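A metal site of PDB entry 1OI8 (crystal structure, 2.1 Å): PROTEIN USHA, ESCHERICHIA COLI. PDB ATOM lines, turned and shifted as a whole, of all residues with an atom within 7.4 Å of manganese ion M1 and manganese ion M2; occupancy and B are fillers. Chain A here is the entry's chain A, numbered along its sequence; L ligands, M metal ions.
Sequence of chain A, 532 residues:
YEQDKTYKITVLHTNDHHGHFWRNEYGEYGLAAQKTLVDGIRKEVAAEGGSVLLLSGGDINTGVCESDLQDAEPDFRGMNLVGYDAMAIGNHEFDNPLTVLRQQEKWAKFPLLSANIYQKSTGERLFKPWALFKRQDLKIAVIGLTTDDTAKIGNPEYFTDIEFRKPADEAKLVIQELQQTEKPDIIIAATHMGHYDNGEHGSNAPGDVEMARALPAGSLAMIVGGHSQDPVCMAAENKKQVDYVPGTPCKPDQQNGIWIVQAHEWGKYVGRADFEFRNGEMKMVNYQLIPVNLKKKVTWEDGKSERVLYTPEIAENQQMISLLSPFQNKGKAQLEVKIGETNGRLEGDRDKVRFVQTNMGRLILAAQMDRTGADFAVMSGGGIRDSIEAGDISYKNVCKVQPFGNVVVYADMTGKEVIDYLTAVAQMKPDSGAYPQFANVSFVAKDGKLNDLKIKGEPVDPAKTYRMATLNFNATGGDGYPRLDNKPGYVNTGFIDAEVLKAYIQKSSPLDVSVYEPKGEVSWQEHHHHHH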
ATOM      1  N   ASN A  15     -34.727  14.795  21.008  1.00  0.00           N
ATOM      2  CA  ASN A  15     -34.168  15.076  22.318  1.00  0.00           C
ATOM      3  C   ASN A  15     -32.664  15.277  22.234  1.00  0.00           C
ATOM      4  O   ASN A  15     -32.027  14.856  21.275  1.00  0.00           O
ATOM      5  CB  ASN A  15     -34.461  13.937  23.266  1.00  0.00           C
ATOM      6  CG  ASN A  15     -33.937  12.605  22.746  1.00  0.00           C
ATOM      7  OD1 ASN A  15     -34.586  11.939  21.933  1.00  0.00           O
ATOM      8  ND2 ASN A  15     -32.743  12.216  23.213  1.00  0.00           N
ATOM      9  N   ASP A  16     -32.118  15.898  23.279  1.00  0.00           N
ATOM     10  CA  ASP A  16     -30.672  16.065  23.408  1.00  0.00           C
ATOM     11  C   ASP A  16     -30.039  16.662  22.171  1.00  0.00           C
ATOM     12  O   ASP A  16     -29.028  16.195  21.653  1.00  0.00           O
ATOM     13  CB  ASP A  16     -30.081  14.722  23.779  1.00  0.00           C
ATOM     14  CG  ASP A  16     -30.483  14.321  25.132  1.00  0.00           C
ATOM     15  OD1 ASP A  16     -29.826  14.791  26.082  1.00  0.00           O
ATOM     16  OD2 ASP A  16     -31.511  13.646  25.325  1.00  0.00           O
ATOM     17  N   HIS A  17     -30.686  17.715  21.704  1.00  0.00           N
ATOM     18  CA  HIS A  17     -30.287  18.500  20.531  1.00  0.00           C
ATOM     19  C   HIS A  17     -28.854  19.051  20.692  1.00  0.00           C
ATOM     20  O   HIS A  17     -28.041  18.990  19.778  1.00  0.00           O
ATOM     21  CB  HIS A  17     -31.322  19.603  20.331  1.00  0.00           C
ATOM     22  CG  HIS A  17     -30.971  20.585  19.273  1.00  0.00           C
ATOM     23  ND1 HIS A  17     -30.956  20.254  17.943  1.00  0.00           N
ATOM     24  CD2 HIS A  17     -30.619  21.896  19.360  1.00  0.00           C
ATOM     25  CE1 HIS A  17     -30.593  21.328  17.248  1.00  0.00           C
ATOM     26  NE2 HIS A  17     -30.403  22.337  18.087  1.00  0.00           N
ATOM     27  N   HIS A  18     -28.562  19.608  21.850  1.00  0.00           N
ATOM     28  CA  HIS A  18     -27.197  19.949  22.246  1.00  0.00           C
ATOM     29  C   HIS A  18     -26.470  20.814  21.249  1.00  0.00           C
ATOM     30  O   HIS A  18     -25.376  20.492  20.812  1.00  0.00           O
ATOM     31  CB  HIS A  18     -26.416  18.696  22.488  1.00  0.00           C
ATOM     32  CG  HIS A  18     -26.666  18.079  23.821  1.00  0.00           C
ATOM     33  ND1 HIS A  18     -26.513  18.766  25.010  1.00  0.00           N
ATOM     34  CD2 HIS A  18     -27.042  16.818  24.158  1.00  0.00           C
ATOM     35  CE1 HIS A  18     -26.767  17.933  26.026  1.00  0.00           C
ATOM     36  NE2 HIS A  18     -27.105  16.766  25.529  1.00  0.00           N
ATOM     37  N   GLY A  57     -37.372  16.139  24.291  1.00  0.00           N
ATOM     38  CA  GLY A  57     -36.977  15.710  25.614  1.00  0.00           C
ATOM     39  C   GLY A  57     -35.873  16.521  26.236  1.00  0.00           C
ATOM     40  O   GLY A  57     -35.279  16.070  27.196  1.00  0.00           O
ATOM     41  N   GLY A  58     -35.556  17.679  25.677  1.00  0.00           N
ATOM     42  CA  GLY A  58     -34.697  18.654  26.343  1.00  0.00           C
ATOM     43  C   GLY A  58     -33.208  18.443  26.048  1.00  0.00           C
ATOM     44  O   GLY A  58     -32.816  17.658  25.160  1.00  0.00           O
ATOM     45  N   ASP A  59     -32.380  19.172  26.796  1.00  0.00           N
ATOM     46  CA  ASP A  59     -30.925  19.246  26.591  1.00  0.00           C
ATOM     47  C   ASP A  59     -30.688  19.828  25.207  1.00  0.00           C
ATOM     48  O   ASP A  59     -30.075  19.223  24.303  1.00  0.00           O
ATOM     49  CB  ASP A  59     -30.243  17.904  26.755  1.00  0.00           C
ATOM     50  CG  ASP A  59     -29.718  17.653  28.148  1.00  0.00           C
ATOM     51  OD1 ASP A  59     -29.985  18.428  29.137  1.00  0.00           O
ATOM     52  OD2 ASP A  59     -28.954  16.693  28.328  1.00  0.00           O
ATOM     53  N   ILE A  60     -31.198  21.039  25.070  1.00  0.00           N
ATOM     54  CA  ILE A  60     -30.967  21.878  23.886  1.00  0.00           C
ATOM     55  C   ILE A  60     -29.571  22.577  24.005  1.00  0.00           C
ATOM     56  O   ILE A  60     -28.823  22.657  23.054  1.00  0.00           O
ATOM     57  CB  ILE A  60     -32.094  22.873  23.746  1.00  0.00           C
ATOM     58  CG1 ILE A  60     -33.491  22.187  23.817  1.00  0.00           C
ATOM     59  CG2 ILE A  60     -31.919  23.769  22.466  1.00  0.00           C
ATOM     60  CD1 ILE A  60     -33.814  21.174  22.767  1.00  0.00           C
ATOM     61  N   ASN A  61     -29.261  23.113  25.185  1.00  0.00           N
ATOM     62  CA  ASN A  61     -27.976  23.709  25.478  1.00  0.00           C
ATOM     63  C   ASN A  61     -26.812  22.720  25.496  1.00  0.00           C
ATOM     64  O   ASN A  61     -26.952  21.581  25.988  1.00  0.00           O
ATOM     65  CB  ASN A  61     -27.986  24.351  26.908  1.00  0.00           C
ATOM     66  CG  ASN A  61     -28.849  25.553  27.012  1.00  0.00           C
ATOM     67  OD1 ASN A  61     -28.386  26.649  26.804  1.00  0.00           O
ATOM     68  ND2 ASN A  61     -30.136  25.348  27.310  1.00  0.00           N
ATOM     69  N   THR A  62     -25.672  23.238  25.025  1.00  0.00           N
ATOM     70  CA  THR A  62     -24.322  22.746  25.263  1.00  0.00           C
ATOM     71  C   THR A  62     -23.942  21.640  24.258  1.00  0.00           C
ATOM     72  O   THR A  62     -24.585  20.624  24.214  1.00  0.00           O
ATOM     73  CB  THR A  62     -24.149  22.279  26.665  1.00  0.00           C
ATOM     74  OG1 THR A  62     -24.476  23.348  27.560  1.00  0.00           O
ATOM     75  CG2 THR A  62     -22.708  21.936  26.993  1.00  0.00           C
ATOM     76  N   GLY A  90     -34.082  19.909  30.352  1.00  0.00           N
ATOM     77  CA  GLY A  90     -33.012  18.992  30.646  1.00  0.00           C
ATOM     78  C   GLY A  90     -32.017  19.530  31.675  1.00  0.00           C
ATOM     79  O   GLY A  90     -32.060  20.693  32.084  1.00  0.00           O
ATOM     80  N   ASN A  91     -31.081  18.683  32.055  1.00  0.00           N
ATOM     81  CA  ASN A  91     -30.070  19.118  33.043  1.00  0.00           C
ATOM     82  C   ASN A  91     -29.166  20.181  32.506  1.00  0.00           C
ATOM     83  O   ASN A  91     -28.805  21.106  33.235  1.00  0.00           O
ATOM     84  CB  ASN A  91     -29.264  17.937  33.600  1.00  0.00           C
ATOM     85  CG  ASN A  91     -28.661  17.080  32.543  1.00  0.00           C
ATOM     86  OD1 ASN A  91     -29.366  16.404  31.867  1.00  0.00           O
ATOM     87  ND2 ASN A  91     -27.297  17.103  32.416  1.00  0.00           N
ATOM     88  N   HIS A  92     -28.882  20.118  31.219  1.00  0.00           N
ATOM     89  CA  HIS A  92     -28.047  21.113  30.601  1.00  0.00           C
ATOM     90  C   HIS A  92     -28.690  22.451  30.391  1.00  0.00           C
ATOM     91  O   HIS A  92     -27.985  23.399  30.070  1.00  0.00           O
ATOM     92  CB  HIS A  92     -27.366  20.604  29.308  1.00  0.00           C
ATOM     93  CG  HIS A  92     -26.293  19.604  29.555  1.00  0.00           C
ATOM     94  ND1 HIS A  92     -24.962  19.939  29.657  1.00  0.00           N
ATOM     95  CD2 HIS A  92     -26.353  18.266  29.763  1.00  0.00           C
ATOM     96  CE1 HIS A  92     -24.243  18.853  29.878  1.00  0.00           C
ATOM     97  NE2 HIS A  92     -25.061  17.817  29.955  1.00  0.00           N
ATOM     98  N   THR A 147     -34.649  14.893  35.368  1.00  0.00           N
ATOM     99  CA  THR A 147     -33.982  13.982  36.249  1.00  0.00           C
ATOM    100  C   THR A 147     -33.510  14.693  37.503  1.00  0.00           C
ATOM    101  O   THR A 147     -32.983  15.806  37.435  1.00  0.00           O
ATOM    102  CB  THR A 147     -32.789  13.277  35.585  1.00  0.00           C
ATOM    103  OG1 THR A 147     -32.087  12.455  36.564  1.00  0.00           O
ATOM    104  CG2 THR A 147     -31.725  14.295  35.117  1.00  0.00           C
ATOM    105  N   THR A 150     -29.787  16.144  38.068  1.00  0.00           N
ATOM    106  CA  THR A 150     -29.378  17.504  37.754  1.00  0.00           C
ATOM    107  C   THR A 150     -28.642  18.166  38.890  1.00  0.00           C
ATOM    108  O   THR A 150     -27.621  18.824  38.671  1.00  0.00           O
ATOM    109  CB  THR A 150     -30.570  18.355  37.373  1.00  0.00           C
ATOM    110  OG1 THR A 150     -31.274  17.749  36.258  1.00  0.00           O
ATOM    111  CG2 THR A 150     -30.082  19.712  36.854  1.00  0.00           C
ATOM    112  N   ILE A 153     -25.152  16.700  39.267  1.00  0.00           N
ATOM    113  CA  ILE A 153     -24.162  16.872  38.230  1.00  0.00           C
ATOM    114  C   ILE A 153     -23.812  18.336  37.925  1.00  0.00           C
ATOM    115  O   ILE A 153     -22.672  18.590  37.556  1.00  0.00           O
ATOM    116  CB  ILE A 153     -24.428  16.102  36.888  1.00  0.00           C
ATOM    117  CG1 ILE A 153     -25.238  16.899  35.935  1.00  0.00           C
ATOM    118  CG2 ILE A 153     -25.100  14.695  37.031  1.00  0.00           C
ATOM    119  CD1 ILE A 153     -24.801  16.641  34.582  1.00  0.00           C
ATOM    120  N   HIS A 192     -36.793  14.243  30.721  1.00  0.00           N
ATOM    121  CA  HIS A 192     -35.381  14.128  30.587  1.00  0.00           C
ATOM    122  C   HIS A 192     -34.872  13.312  31.757  1.00  0.00           C
ATOM    123  O   HIS A 192     -34.389  13.867  32.762  1.00  0.00           O
ATOM    124  CB  HIS A 192     -34.768  15.496  30.596  1.00  0.00           C
ATOM    125  CG  HIS A 192     -33.368  15.517  30.111  1.00  0.00           C
ATOM    126  ND1 HIS A 192     -33.054  15.910  28.836  1.00  0.00           N
ATOM    127  CD2 HIS A 192     -32.221  15.029  30.648  1.00  0.00           C
ATOM    128  CE1 HIS A 192     -31.750  15.773  28.645  1.00  0.00           C
ATOM    129  NE2 HIS A 192     -31.214  15.262  29.733  1.00  0.00           N
ATOM    130  N   MET A 193     -35.041  11.988  31.619  1.00  0.00           N
ATOM    131  CA  MET A 193     -34.787  11.035  32.725  1.00  0.00           C
ATOM    132  C   MET A 193     -33.934   9.808  32.426  1.00  0.00           C
ATOM    133  O   MET A 193     -33.299   9.292  33.340  1.00  0.00           O
ATOM    134  CB  MET A 193     -36.116  10.574  33.327  1.00  0.00           C
ATOM    135  CG  MET A 193     -36.801  11.633  34.129  1.00  0.00           C
ATOM    136  SD  MET A 193     -38.590  11.207  34.385  1.00  0.00           S
ATOM    137  CE  MET A 193     -38.458   9.629  35.203  1.00  0.00           C
ATOM    138  N   GLY A 226     -35.379  11.294  26.948  1.00  0.00           N
ATOM    139  CA  GLY A 226     -34.104  11.893  26.661  1.00  0.00           C
ATOM    140  C   GLY A 226     -33.081  11.471  27.690  1.00  0.00           C
ATOM    141  O   GLY A 226     -33.287  10.496  28.433  1.00  0.00           O
ATOM    142  N   HIS A 227     -31.969  12.178  27.653  1.00  0.00           N
ATOM    143  CA  HIS A 227     -30.901  12.180  28.685  1.00  0.00           C
ATOM    144  C   HIS A 227     -29.957  11.018  28.552  1.00  0.00           C
ATOM    145  O   HIS A 227     -28.771  11.215  28.481  1.00  0.00           O
ATOM    146  CB  HIS A 227     -31.462  12.184  30.091  1.00  0.00           C
ATOM    147  CG  HIS A 227     -30.424  12.268  31.182  1.00  0.00           C
ATOM    148  ND1 HIS A 227     -29.681  13.399  31.441  1.00  0.00           N
ATOM    149  CD2 HIS A 227     -30.021  11.329  32.087  1.00  0.00           C
ATOM    150  CE1 HIS A 227     -28.865  13.167  32.469  1.00  0.00           C
ATOM    151  NE2 HIS A 227     -29.091  11.934  32.903  1.00  0.00           N
ATOM    152  N   SER A 228     -30.472   9.792  28.494  1.00  0.00           N
ATOM    153  CA  SER A 228     -29.560   8.652  28.258  1.00  0.00           C
ATOM    154  C   SER A 228     -28.931   8.725  26.857  1.00  0.00           C
ATOM    155  O   SER A 228     -27.808   8.227  26.634  1.00  0.00           O
ATOM    156  CB  SER A 228     -30.272   7.316  28.507  1.00  0.00           C
ATOM    157  OG  SER A 228     -31.485   7.187  27.803  1.00  0.00           O
ATOM    158  N   GLN A 229     -29.602   9.406  25.941  1.00  0.00           N
ATOM    159  CA  GLN A 229     -29.144   9.536  24.566  1.00  0.00           C
ATOM    160  C   GLN A 229     -29.054   8.181  23.875  1.00  0.00           C
ATOM    161  O   GLN A 229     -28.010   7.759  23.455  1.00  0.00           O
ATOM    162  CB  GLN A 229     -27.853  10.402  24.457  1.00  0.00           C
ATOM    163  CG  GLN A 229     -28.090  11.885  24.910  1.00  0.00           C
ATOM    164  CD  GLN A 229     -26.878  12.842  24.849  1.00  0.00           C
ATOM    165  OE1 GLN A 229     -26.792  13.652  25.734  1.00  0.00           O
ATOM    166  NE2 GLN A 229     -26.000  12.781  23.793  1.00  0.00           N
ATOM    167  N   HIS A 264     -32.367   9.299  20.249  1.00  0.00           N
ATOM    168  CA  HIS A 264     -30.887   9.391  20.313  1.00  0.00           C
ATOM    169  C   HIS A 264     -30.393  10.783  20.678  1.00  0.00           C
ATOM    170  O   HIS A 264     -30.306  11.110  21.888  1.00  0.00           O
ATOM    171  CB  HIS A 264     -30.195   8.806  19.076  1.00  0.00           C
ATOM    172  CG  HIS A 264     -28.753   8.423  19.252  1.00  0.00           C
ATOM    173  ND1 HIS A 264     -27.977   8.006  18.195  1.00  0.00           N
ATOM    174  CD2 HIS A 264     -27.975   8.309  20.359  1.00  0.00           C
ATOM    175  CE1 HIS A 264     -26.760   7.718  18.627  1.00  0.00           C
ATOM    176  NE2 HIS A 264     -26.736   7.864  19.938  1.00  0.00           N
ATOM    177  N   GLU A 265     -30.050  11.595  19.704  1.00  0.00           N
ATOM    178  CA  GLU A 265     -29.416  12.868  20.015  1.00  0.00           C
ATOM    179  C   GLU A 265     -29.179  13.710  18.788  1.00  0.00           C
ATOM    180  O   GLU A 265     -29.097  13.196  17.656  1.00  0.00           O
ATOM    181  CB  GLU A 265     -28.049  12.631  20.712  1.00  0.00           C
ATOM    182  CG  GLU A 265     -27.020  11.991  19.772  1.00  0.00           C
ATOM    183  CD  GLU A 265     -25.776  11.394  20.429  1.00  0.00           C
ATOM    184  OE1 GLU A 265     -25.677  11.203  21.671  1.00  0.00           O
ATOM    185  OE2 GLU A 265     -24.912  11.015  19.643  1.00  0.00           O
ATOM    186  N   TRP A 266     -28.988  15.006  19.048  1.00  0.00           N
ATOM    187  CA  TRP A 266     -28.390  15.982  18.101  1.00  0.00           C
ATOM    188  C   TRP A 266     -29.171  16.263  16.845  1.00  0.00           C
ATOM    189  O   TRP A 266     -28.626  16.718  15.807  1.00  0.00           O
ATOM    190  CB  TRP A 266     -26.994  15.589  17.690  1.00  0.00           C
ATOM    191  CG  TRP A 266     -25.967  15.341  18.739  1.00  0.00           C
ATOM    192  CD1 TRP A 266     -26.066  15.577  20.065  1.00  0.00           C
ATOM    193  CD2 TRP A 266     -24.640  14.884  18.513  1.00  0.00           C
ATOM    194  NE1 TRP A 266     -24.889  15.267  20.701  1.00  0.00           N
ATOM    195  CE2 TRP A 266     -23.993  14.823  19.774  1.00  0.00           C
ATOM    196  CE3 TRP A 266     -23.938  14.497  17.382  1.00  0.00           C
ATOM    197  CZ2 TRP A 266     -22.694  14.362  19.938  1.00  0.00           C
ATOM    198  CZ3 TRP A 266     -22.611  14.030  17.527  1.00  0.00           C
ATOM    199  CH2 TRP A 266     -22.013  13.960  18.792  1.00  0.00           C
HETATM  200  C1  LIG L   1     -26.843  14.534  29.391  1.00  0.00           C
HETATM  201  O1  LIG L   1     -28.002  13.970  28.798  1.00  0.00           O
HETATM  202  O2  LIG L   1     -25.783  14.853  28.673  1.00  0.00           O
HETATM  203  O3  LIG L   1     -26.845  14.975  30.637  1.00  0.00           O
HETATM  204 MN    MN M   1     -29.135  15.083  30.139  1.00  0.00          MN
HETATM  205 MN    MN M   2     -27.906  15.202  26.954  1.00  0.00          MN
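N of His 227 is in hydrogen-bond range of OD2 of Asp 16 (2.8 Å).
The backbone carbonyl oxygen (O) of Ile 60 sits close to the backbone NH (N) of His 18 (3.3 Å).
The side-chain carboxylate of Asp 16 sits at hydrogen-bond distance from the side-chain amide nitrogen of Asn 15, at 2.8 Å.
A ring nitrogen (ND1) of His 18 lies within hydrogen-bond range of the backbone carbonyl oxygen of Thr 62 (2.8 Å).
O of Asp 16 lies within hydrogen-bond range of N of Trp 266, 2.9 Å away.
N of Asp 16 is in hydrogen-bond range of O of Gly 58 (2.7 Å).
The backbone NH of His 92 sits at hydrogen-bond distance from the side-chain carboxylate of Asp 59.
The backbone NH (N) of Thr 147 is in hydrogen-bond range of the backbone carbonyl oxygen (O) of His 192.
Of the 25 residues printed, 4 come within 4 Å of manganese ion M1.
Manganese ion M1 is bound by an oxygen (O1) of the ligand (2.1 Å), a ring nitrogen (NE2) of His 192 (2.1 Å), the side-chain amide oxygen (OD1) of Asn 91 (2.2 Å), a ring nitrogen (ND1) of His 227 (2.2 Å), an oxygen (O3) of the ligand (2.3 Å) and the side-chain carboxylate (OD2) of Asp 59 (2.4 Å).
Manganese ion M2 is bound by OD1 of Asp 16, O1 of the ligand, NE2 of His 18, OE1 of Gln 229 and OD2 of Asp 59.
Manganese ion M2 has five donor atoms within binding distance.
Slightly farther from manganese ion M2 lies O2 of the ligand (2.8 Å).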
